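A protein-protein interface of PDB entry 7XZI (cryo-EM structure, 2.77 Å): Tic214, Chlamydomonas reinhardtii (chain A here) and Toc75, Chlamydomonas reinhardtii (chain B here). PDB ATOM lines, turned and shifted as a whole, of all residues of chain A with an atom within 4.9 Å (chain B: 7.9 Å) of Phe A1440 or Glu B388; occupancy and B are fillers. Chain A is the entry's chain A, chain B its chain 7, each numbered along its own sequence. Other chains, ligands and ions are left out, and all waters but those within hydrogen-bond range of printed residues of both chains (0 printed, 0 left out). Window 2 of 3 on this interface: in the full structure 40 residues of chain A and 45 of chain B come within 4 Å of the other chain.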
ATOM      1  N   ARG A1366      21.445 -20.912   7.471  1.00  0.00           N
ATOM      2  CA  ARG A1366      22.525 -20.283   8.216  1.00  0.00           C
ATOM      3  C   ARG A1366      23.841 -20.550   7.502  1.00  0.00           C
ATOM      4  O   ARG A1366      23.951 -21.468   6.684  1.00  0.00           O
ATOM      5  CB  ARG A1366      22.569 -20.788   9.664  1.00  0.00           C
ATOM      6  CG  ARG A1366      22.580 -22.302   9.798  1.00  0.00           C
ATOM      7  CD  ARG A1366      22.238 -22.748  11.215  1.00  0.00           C
ATOM      8  NE  ARG A1366      23.037 -22.073  12.227  1.00  0.00           N
ATOM      9  CZ  ARG A1366      22.587 -21.104  13.018  1.00  0.00           C
ATOM     10  NH1 ARG A1366      21.337 -20.677  12.944  1.00  0.00           N
ATOM     11  NH2 ARG A1366      23.411 -20.551  13.902  1.00  0.00           N
ATOM     12  N   TYR A1367      24.839 -19.723   7.824  1.00  0.00           N
ATOM     13  CA  TYR A1367      26.177 -19.804   7.234  1.00  0.00           C
ATOM     14  C   TYR A1367      26.143 -19.646   5.716  1.00  0.00           C
ATOM     15  O   TYR A1367      26.987 -20.198   5.005  1.00  0.00           O
ATOM     16  CB  TYR A1367      26.881 -21.109   7.617  1.00  0.00           C
ATOM     17  CG  TYR A1367      26.901 -21.382   9.103  1.00  0.00           C
ATOM     18  CD1 TYR A1367      27.780 -20.710   9.941  1.00  0.00           C
ATOM     19  CD2 TYR A1367      26.044 -22.316   9.666  1.00  0.00           C
ATOM     20  CE1 TYR A1367      27.800 -20.959  11.301  1.00  0.00           C
ATOM     21  CE2 TYR A1367      26.054 -22.569  11.023  1.00  0.00           C
ATOM     22  CZ  TYR A1367      26.935 -21.889  11.836  1.00  0.00           C
ATOM     23  OH  TYR A1367      26.948 -22.142  13.188  1.00  0.00           O
ATOM     24  N   HIS A1438      31.916 -22.369  12.426  1.00  0.00           N
ATOM     25  CA  HIS A1438      30.959 -23.474  12.514  1.00  0.00           C
ATOM     26  C   HIS A1438      31.049 -24.210  13.849  1.00  0.00           C
ATOM     27  O   HIS A1438      30.841 -25.424  13.916  1.00  0.00           O
ATOM     28  CB  HIS A1438      31.133 -24.455  11.350  1.00  0.00           C
ATOM     29  CG  HIS A1438      30.983 -23.827   9.999  1.00  0.00           C
ATOM     30  ND1 HIS A1438      29.772 -23.379   9.517  1.00  0.00           N
ATOM     31  CD2 HIS A1438      31.891 -23.576   9.027  1.00  0.00           C
ATOM     32  CE1 HIS A1438      29.940 -22.877   8.308  1.00  0.00           C
ATOM     33  NE2 HIS A1438      31.217 -22.984   7.986  1.00  0.00           N
ATOM     34  N   GLN A1439      31.358 -23.483  14.925  1.00  0.00           N
ATOM     35  CA  GLN A1439      31.381 -24.088  16.253  1.00  0.00           C
ATOM     36  C   GLN A1439      29.971 -24.336  16.777  1.00  0.00           C
ATOM     37  O   GLN A1439      29.720 -25.350  17.444  1.00  0.00           O
ATOM     38  CB  GLN A1439      32.168 -23.202  17.221  1.00  0.00           C
ATOM     39  CG  GLN A1439      32.152 -23.682  18.665  1.00  0.00           C
ATOM     40  CD  GLN A1439      32.778 -25.054  18.837  1.00  0.00           C
ATOM     41  OE1 GLN A1439      33.680 -25.436  18.091  1.00  0.00           O
ATOM     42  NE2 GLN A1439      32.298 -25.802  19.822  1.00  0.00           N
ATOM     43  N   PHE A1440      29.043 -23.421  16.489  1.00  0.00           N
ATOM     44  CA  PHE A1440      27.664 -23.598  16.934  1.00  0.00           C
ATOM     45  C   PHE A1440      27.032 -24.835  16.312  1.00  0.00           C
ATOM     46  O   PHE A1440      26.225 -25.509  16.962  1.00  0.00           O
ATOM     47  CB  PHE A1440      26.841 -22.354  16.603  1.00  0.00           C
ATOM     48  CG  PHE A1440      25.397 -22.460  17.003  1.00  0.00           C
ATOM     49  CD1 PHE A1440      25.011 -22.258  18.317  1.00  0.00           C
ATOM     50  CD2 PHE A1440      24.425 -22.756  16.062  1.00  0.00           C
ATOM     51  CE1 PHE A1440      23.683 -22.354  18.687  1.00  0.00           C
ATOM     52  CE2 PHE A1440      23.095 -22.853  16.426  1.00  0.00           C
ATOM     53  CZ  PHE A1440      22.724 -22.651  17.740  1.00  0.00           C
ATOM     54  N   SER A1441      27.379 -25.149  15.062  1.00  0.00           N
ATOM     55  CA  SER A1441      26.881 -26.376  14.446  1.00  0.00           C
ATOM     56  C   SER A1441      27.382 -27.607  15.189  1.00  0.00           C
ATOM     57  O   SER A1441      26.628 -28.563  15.403  1.00  0.00           O
ATOM     58  CB  SER A1441      27.295 -26.432  12.976  1.00  0.00           C
ATOM     59  OG  SER A1441      26.741 -25.351  12.248  1.00  0.00           O
ATOM     60  N   ARG A1442      28.657 -27.604  15.586  1.00  0.00           N
ATOM     61  CA  ARG A1442      29.195 -28.724  16.354  1.00  0.00           C
ATOM     62  C   ARG A1442      28.512 -28.846  17.710  1.00  0.00           C
ATOM     63  O   ARG A1442      28.211 -29.956  18.164  1.00  0.00           O
ATOM     64  CB  ARG A1442      30.707 -28.567  16.519  1.00  0.00           C
ATOM     65  CG  ARG A1442      31.494 -28.820  15.242  1.00  0.00           C
ATOM     66  CD  ARG A1442      32.989 -28.653  15.461  1.00  0.00           C
ATOM     67  NE  ARG A1442      33.382 -27.252  15.538  1.00  0.00           N
ATOM     68  CZ  ARG A1442      33.759 -26.522  14.494  1.00  0.00           C
ATOM     69  NH1 ARG A1442      33.798 -27.032  13.273  1.00  0.00           N
ATOM     70  NH2 ARG A1442      34.105 -25.253  14.681  1.00  0.00           N
ATOM     71  N   ASN A1443      28.259 -27.714  18.372  1.00  0.00           N
ATOM     72  CA  ASN A1443      27.543 -27.751  19.644  1.00  0.00           C
ATOM     73  C   ASN A1443      26.128 -28.290  19.466  1.00  0.00           C
ATOM     74  O   ASN A1443      25.647 -29.083  20.285  1.00  0.00           O
ATOM     75  CB  ASN A1443      27.512 -26.357  20.272  1.00  0.00           C
ATOM     76  CG  ASN A1443      28.895 -25.843  20.620  1.00  0.00           C
ATOM     77  OD1 ASN A1443      29.904 -26.368  20.148  1.00  0.00           O
ATOM     78  ND2 ASN A1443      28.950 -24.808  21.451  1.00  0.00           N
ATOM     79  N   HIS A1444      25.446 -27.872  18.398  1.00  0.00           N
ATOM     80  CA  HIS A1444      24.103 -28.375  18.131  1.00  0.00           C
ATOM     81  C   HIS A1444      24.122 -29.874  17.862  1.00  0.00           C
ATOM     82  O   HIS A1444      23.237 -30.605  18.319  1.00  0.00           O
ATOM     83  CB  HIS A1444      23.485 -27.625  16.951  1.00  0.00           C
ATOM     84  CG  HIS A1444      22.003 -27.798  16.836  1.00  0.00           C
ATOM     85  ND1 HIS A1444      21.231 -28.291  17.866  1.00  0.00           N
ATOM     86  CD2 HIS A1444      21.150 -27.545  15.815  1.00  0.00           C
ATOM     87  CE1 HIS A1444      19.967 -28.333  17.485  1.00  0.00           C
ATOM     88  NE2 HIS A1444      19.891 -27.886  16.244  1.00  0.00           N
ATOM     89  N   VAL B 331      19.859 -10.946  16.839  1.00  0.00           N
ATOM     90  CA  VAL B 331      19.246 -12.227  17.164  1.00  0.00           C
ATOM     91  C   VAL B 331      20.240 -13.080  17.937  1.00  0.00           C
ATOM     92  O   VAL B 331      21.460 -12.926  17.806  1.00  0.00           O
ATOM     93  CB  VAL B 331      18.764 -12.973  15.899  1.00  0.00           C
ATOM     94  CG1 VAL B 331      17.637 -12.204  15.224  1.00  0.00           C
ATOM     95  CG2 VAL B 331      19.921 -13.189  14.936  1.00  0.00           C
ATOM     96  N   ARG B 332      19.704 -13.984  18.754  1.00  0.00           N
ATOM     97  CA  ARG B 332      20.509 -14.920  19.532  1.00  0.00           C
ATOM     98  C   ARG B 332      19.877 -16.300  19.419  1.00  0.00           C
ATOM     99  O   ARG B 332      18.691 -16.466  19.770  1.00  0.00           O
ATOM    100  CB  ARG B 332      20.604 -14.482  20.996  1.00  0.00           C
ATOM    101  CG  ARG B 332      21.022 -15.590  21.948  1.00  0.00           C
ATOM    102  CD  ARG B 332      20.989 -15.116  23.391  1.00  0.00           C
ATOM    103  NE  ARG B 332      21.107 -16.220  24.331  1.00  0.00           N
ATOM    104  CZ  ARG B 332      20.075 -16.895  24.828  1.00  0.00           C
ATOM    105  NH1 ARG B 332      18.831 -16.603  24.488  1.00  0.00           N
ATOM    106  NH2 ARG B 332      20.300 -17.886  25.685  1.00  0.00           N
ATOM    107  N   PRO B 333      20.601 -17.308  18.929  1.00  0.00           N
ATOM    108  CA  PRO B 333      20.047 -18.664  18.872  1.00  0.00           C
ATOM    109  C   PRO B 333      20.321 -19.446  20.147  1.00  0.00           C
ATOM    110  O   PRO B 333      21.398 -19.369  20.742  1.00  0.00           O
ATOM    111  CB  PRO B 333      20.781 -19.291  17.675  1.00  0.00           C
ATOM    112  CG  PRO B 333      21.810 -18.254  17.213  1.00  0.00           C
ATOM    113  CD  PRO B 333      21.926 -17.238  18.299  1.00  0.00           C
ATOM    114  N   LYS B 334      19.319 -20.213  20.570  1.00  0.00           N
ATOM    115  CA  LYS B 334      19.431 -21.028  21.768  1.00  0.00           C
ATOM    116  C   LYS B 334      19.966 -22.416  21.418  1.00  0.00           C
ATOM    117  O   LYS B 334      20.180 -22.756  20.252  1.00  0.00           O
ATOM    118  CB  LYS B 334      18.082 -21.115  22.480  1.00  0.00           C
ATOM    119  CG  LYS B 334      17.624 -19.805  23.101  1.00  0.00           C
ATOM    120  CD  LYS B 334      16.317 -19.974  23.859  1.00  0.00           C
ATOM    121  CE  LYS B 334      15.164 -20.268  22.914  1.00  0.00           C
ATOM    122  NZ  LYS B 334      14.912 -19.133  21.984  1.00  0.00           N
ATOM    123  N   LEU B 335      20.186 -23.231  22.448  1.00  0.00           N
ATOM    124  CA  LEU B 335      20.719 -24.580  22.290  1.00  0.00           C
ATOM    125  C   LEU B 335      19.756 -25.570  22.926  1.00  0.00           C
ATOM    126  O   LEU B 335      19.439 -25.453  24.114  1.00  0.00           O
ATOM    127  CB  LEU B 335      22.109 -24.703  22.922  1.00  0.00           C
ATOM    128  CG  LEU B 335      23.291 -24.224  22.078  1.00  0.00           C
ATOM    129  CD1 LEU B 335      24.561 -24.168  22.912  1.00  0.00           C
ATOM    130  CD2 LEU B 335      23.481 -25.137  20.878  1.00  0.00           C
ATOM    131  N   THR B 336      19.304 -26.542  22.140  1.00  0.00           N
ATOM    132  CA  THR B 336      18.403 -27.578  22.626  1.00  0.00           C
ATOM    133  C   THR B 336      18.414 -28.733  21.634  1.00  0.00           C
ATOM    134  O   THR B 336      18.924 -28.616  20.517  1.00  0.00           O
ATOM    135  CB  THR B 336      16.980 -27.045  22.825  1.00  0.00           C
ATOM    136  OG1 THR B 336      16.142 -28.089  23.334  1.00  0.00           O
ATOM    137  CG2 THR B 336      16.409 -26.543  21.508  1.00  0.00           C
ATOM    138  N   LEU B 341      15.783 -24.754  15.779  1.00  0.00           N
ATOM    139  CA  LEU B 341      16.376 -23.652  16.524  1.00  0.00           C
ATOM    140  C   LEU B 341      15.360 -22.543  16.764  1.00  0.00           C
ATOM    141  O   LEU B 341      14.543 -22.223  15.896  1.00  0.00           O
ATOM    142  CB  LEU B 341      17.589 -23.101  15.773  1.00  0.00           C
ATOM    143  CG  LEU B 341      18.760 -24.066  15.589  1.00  0.00           C
ATOM    144  CD1 LEU B 341      19.889 -23.401  14.819  1.00  0.00           C
ATOM    145  CD2 LEU B 341      19.251 -24.572  16.936  1.00  0.00           C
ATOM    146  N   GLU B 342      15.418 -21.956  17.957  1.00  0.00           N
ATOM    147  CA  GLU B 342      14.592 -20.818  18.324  1.00  0.00           C
ATOM    148  C   GLU B 342      15.484 -19.610  18.571  1.00  0.00           C
ATOM    149  O   GLU B 342      16.608 -19.739  19.065  1.00  0.00           O
ATOM    150  CB  GLU B 342      13.750 -21.116  19.572  1.00  0.00           C
ATOM    151  N   TYR B 343      14.974 -18.431  18.227  1.00  0.00           N
ATOM    152  CA  TYR B 343      15.744 -17.200  18.294  1.00  0.00           C
ATOM    153  C   TYR B 343      15.119 -16.226  19.282  1.00  0.00           C
ATOM    154  O   TYR B 343      13.895 -16.172  19.442  1.00  0.00           O
ATOM    155  CB  TYR B 343      15.847 -16.530  16.918  1.00  0.00           C
ATOM    156  CG  TYR B 343      16.706 -17.281  15.927  1.00  0.00           C
ATOM    157  CD1 TYR B 343      18.076 -17.065  15.865  1.00  0.00           C
ATOM    158  CD2 TYR B 343      16.147 -18.199  15.050  1.00  0.00           C
ATOM    159  CE1 TYR B 343      18.866 -17.745  14.960  1.00  0.00           C
ATOM    160  CE2 TYR B 343      16.929 -18.886  14.141  1.00  0.00           C
ATOM    161  CZ  TYR B 343      18.288 -18.655  14.101  1.00  0.00           C
ATOM    162  OH  TYR B 343      19.071 -19.335  13.198  1.00  0.00           O
ATOM    163  N   PHE B 382      31.816  -8.437   8.842  1.00  0.00           N
ATOM    164  CA  PHE B 382      32.371  -9.625   9.474  1.00  0.00           C
ATOM    165  C   PHE B 382      33.837  -9.467   9.849  1.00  0.00           C
ATOM    166  O   PHE B 382      34.408 -10.386  10.448  1.00  0.00           O
ATOM    167  CB  PHE B 382      32.198 -10.838   8.558  1.00  0.00           C
ATOM    168  CG  PHE B 382      32.139 -12.146   9.293  1.00  0.00           C
ATOM    169  CD1 PHE B 382      31.007 -12.496  10.012  1.00  0.00           C
ATOM    170  CD2 PHE B 382      33.207 -13.026   9.265  1.00  0.00           C
ATOM    171  CE1 PHE B 382      30.946 -13.695  10.693  1.00  0.00           C
ATOM    172  CE2 PHE B 382      33.151 -14.228   9.942  1.00  0.00           C
ATOM    173  CZ  PHE B 382      32.018 -14.563  10.657  1.00  0.00           C
ATOM    174  N   CYS B 384      34.799  -7.808  12.187  1.00  0.00           N
ATOM    175  CA  CYS B 384      34.755  -7.913  13.640  1.00  0.00           C
ATOM    176  C   CYS B 384      34.741  -9.381  14.052  1.00  0.00           C
ATOM    177  O   CYS B 384      33.912 -10.161  13.570  1.00  0.00           O
ATOM    178  CB  CYS B 384      33.524  -7.191  14.182  1.00  0.00           C
ATOM    179  SG  CYS B 384      33.435  -5.440  13.741  1.00  0.00           S
ATOM    180  N   GLY B 385      35.659  -9.757  14.943  1.00  0.00           N
ATOM    181  CA  GLY B 385      35.751 -11.146  15.360  1.00  0.00           C
ATOM    182  C   GLY B 385      34.677 -11.560  16.346  1.00  0.00           C
ATOM    183  O   GLY B 385      34.380 -12.752  16.477  1.00  0.00           O
ATOM    184  N   LEU B 386      34.085 -10.595  17.052  1.00  0.00           N
ATOM    185  CA  LEU B 386      33.068 -10.911  18.050  1.00  0.00           C
ATOM    186  C   LEU B 386      31.836 -11.535  17.405  1.00  0.00           C
ATOM    187  O   LEU B 386      31.256 -12.489  17.936  1.00  0.00           O
ATOM    188  CB  LEU B 386      32.690  -9.649  18.828  1.00  0.00           C
ATOM    189  N   LEU B 387      31.420 -11.004  16.258  1.00  0.00           N
ATOM    190  CA  LEU B 387      30.209 -11.485  15.604  1.00  0.00           C
ATOM    191  C   LEU B 387      30.384 -12.916  15.114  1.00  0.00           C
ATOM    192  O   LEU B 387      31.456 -13.306  14.643  1.00  0.00           O
ATOM    193  CB  LEU B 387      29.842 -10.570  14.436  1.00  0.00           C
ATOM    194  N   GLU B 388      29.315 -13.705  15.231  1.00  0.00           N
ATOM    195  CA  GLU B 388      29.301 -15.094  14.793  1.00  0.00           C
ATOM    196  C   GLU B 388      28.755 -15.260  13.381  1.00  0.00           C
ATOM    197  O   GLU B 388      29.433 -15.819  12.515  1.00  0.00           O
ATOM    198  CB  GLU B 388      28.474 -15.945  15.764  1.00  0.00           C
ATOM    199  CG  GLU B 388      28.354 -17.404  15.366  1.00  0.00           C
ATOM    200  CD  GLU B 388      27.187 -18.095  16.043  1.00  0.00           C
ATOM    201  OE1 GLU B 388      26.073 -17.528  16.032  1.00  0.00           O
ATOM    202  OE2 GLU B 388      27.385 -19.197  16.593  1.00  0.00           O
ATOM    203  N   ASP B 389      27.534 -14.789  13.132  1.00  0.00           N
ATOM    204  CA  ASP B 389      26.886 -14.960  11.841  1.00  0.00           C
ATOM    205  C   ASP B 389      26.285 -13.640  11.378  1.00  0.00           C
ATOM    206  O   ASP B 389      25.796 -12.844  12.184  1.00  0.00           O
ATOM    207  CB  ASP B 389      25.794 -16.038  11.901  1.00  0.00           C
ATOM    208  CG  ASP B 389      25.303 -16.450  10.526  1.00  0.00           C
ATOM    209  OD1 ASP B 389      25.901 -16.012   9.521  1.00  0.00           O
ATOM    210  OD2 ASP B 389      24.318 -17.215  10.451  1.00  0.00           O
ATOM    211  N   ILE B 390      26.318 -13.425  10.061  1.00  0.00           N
ATOM    212  CA  ILE B 390      25.784 -12.223   9.437  1.00  0.00           C
ATOM    213  C   ILE B 390      24.937 -12.634   8.238  1.00  0.00           C
ATOM    214  O   ILE B 390      25.134 -13.695   7.640  1.00  0.00           O
ATOM    215  CB  ILE B 390      26.907 -11.247   9.011  1.00  0.00           C
ATOM    216  CG1 ILE B 390      26.341  -9.862   8.681  1.00  0.00           C
ATOM    217  CG2 ILE B 390      27.688 -11.802   7.827  1.00  0.00           C
ATOM    218  CD1 ILE B 390      25.696  -9.167   9.857  1.00  0.00           C
ATOM    219  N   CYS B 410      22.330 -10.038  12.433  1.00  0.00           N
ATOM    220  CA  CYS B 410      23.605 -10.407  13.030  1.00  0.00           C
ATOM    221  C   CYS B 410      23.368 -11.196  14.306  1.00  0.00           C
ATOM    222  O   CYS B 410      22.444 -10.898  15.069  1.00  0.00           O
ATOM    223  CB  CYS B 410      24.462  -9.169  13.329  1.00  0.00           C
ATOM    224  SG  CYS B 410      23.684  -7.967  14.432  1.00  0.00           S
ATOM    225  N   GLU B 411      24.210 -12.202  14.533  1.00  0.00           N
ATOM    226  CA  GLU B 411      24.154 -13.026  15.731  1.00  0.00           C
ATOM    227  C   GLU B 411      25.561 -13.212  16.279  1.00  0.00           C
ATOM    228  O   GLU B 411      26.502 -13.461  15.520  1.00  0.00           O
ATOM    229  CB  GLU B 411      23.516 -14.391  15.444  1.00  0.00           C
ATOM    230  N   GLU B 412      25.693 -13.096  17.601  1.00  0.00           N
ATOM    231  CA  GLU B 412      26.973 -13.219  18.279  1.00  0.00           C
ATOM    232  C   GLU B 412      27.236 -14.674  18.663  1.00  0.00           C
ATOM    233  O   GLU B 412      26.425 -15.570  18.413  1.00  0.00           O
ATOM    234  CB  GLU B 412      27.013 -12.310  19.506  1.00  0.00           C
ATOM    235  N   VAL B 413      28.393 -14.918  19.279  1.00  0.00           N
ATOM    236  CA  VAL B 413      28.845 -16.261  19.624  1.00  0.00           C
ATOM    237  C   VAL B 413      28.949 -16.386  21.139  1.00  0.00           C
ATOM    238  O   VAL B 413      29.417 -15.465  21.820  1.00  0.00           O
ATOM    239  CB  VAL B 413      30.192 -16.588  18.944  1.00  0.00           C
ATOM    240  CG1 VAL B 413      31.241 -15.537  19.281  1.00  0.00           C
ATOM    241  CG2 VAL B 413      30.670 -17.981  19.334  1.00  0.00           C
ATOM    242  N   GLN B 414      28.493 -17.523  21.665  1.00  0.00           N
ATOM    243  CA  GLN B 414      28.636 -17.829  23.084  1.00  0.00           C
ATOM    244  C   GLN B 414      29.946 -18.571  23.313  1.00  0.00           C
ATOM    245  O   GLN B 414      30.117 -19.676  22.781  1.00  0.00           O
ATOM    246  CB  GLN B 414      27.467 -18.667  23.575  1.00  0.00           C
ATOM    247  CG  GLN B 414      26.132 -17.929  23.641  1.00  0.00           C
ATOM    248  CD  GLN B 414      25.442 -17.814  22.292  1.00  0.00           C
ATOM    249  OE1 GLN B 414      26.087 -17.823  21.244  1.00  0.00           O
ATOM    250  NE2 GLN B 414      24.118 -17.708  22.316  1.00  0.00           N
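The side-chain hydroxyl of Tyr B343 is in hydrogen-bond range of the guanidinium group of Arg A1366 (2.6 Å).
The backbone NH (N) of Lys B334 lies within hydrogen-bond range of the backbone carbonyl oxygen (O) of Glu B342, 3.1 Å away. The backbone NH (N) of Glu B388 sits at hydrogen-bond distance from the backbone carbonyl oxygen (O) of Glu B411, at 2.8 Å. The backbone NH (N) of Glu B411 is in hydrogen-bond range of the backbone carbonyl oxygen (O) of Asp B389. The side-chain hydroxyl (OH) of Tyr A1367 sits close to the side-chain hydroxyl (OG) of Ser A1441 (3.4 Å).
Among the printed residues, pairs that only touch across the chains: Phe A1440 with Glu B388 (3.2 Å), His A1444 with Thr B336 (3.2 Å), His A1444 with Leu B341 (3.4 Å), Phe A1440 with Leu B335 (3.5 Å), Phe A1440 with Lys B334 (3.6 Å), Arg A1366 with Leu B341 (3.6 Å), Phe A1440 with Leu B341 (3.6 Å), Tyr A1367 with Asp B389 (3.7 Å) and Phe A1440 with Pro B333 (3.9 Å).
Of chain B, only Pro B333 (3.9 Å), Lys B334 (3.6 Å), Leu B335 (3.5 Å), Leu B341 (3.6 Å) and Glu B388 (3.2 Å) come within 4 Å of Phe A1440. Of the printed residues of chain A, Leu B335 touches Phe A1440 (3.5 Å). Printed residues of chain A within 4 Å of Leu B341: Arg A1366, Phe A1440 and His A1444. Cys B384 touches none of the printed residues of chain A. Glu B388 touches one residue of chain A. The nearest printed residue of chain A that does not touch Asp B389 is Arg A1366 (4.1 Å).
Of the 22 printed residues of chain B, 8 touch a printed residue of chain A. Printed residues of chain B that touch a printed residue of chain A: Pro B333, Lys B334, Leu B335, Thr B336, Leu B341, Tyr B343, Glu B388 and Asp B389. Along chain B the printed residues that touch a printed residue of chain A span positions 333 to 389. Of the 9 printed residues of chain A, 4 touch a printed residue of chain B. Along chain A the printed residues that touch a printed residue of chain B span positions 1366 to 1444. Among the printed residues, 10 pairs touch across the chains. Among the printed residues, no Asp or Glu carboxylate lies within 4 Å of a Lys or Arg side-chain nitrogen of the other chain.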
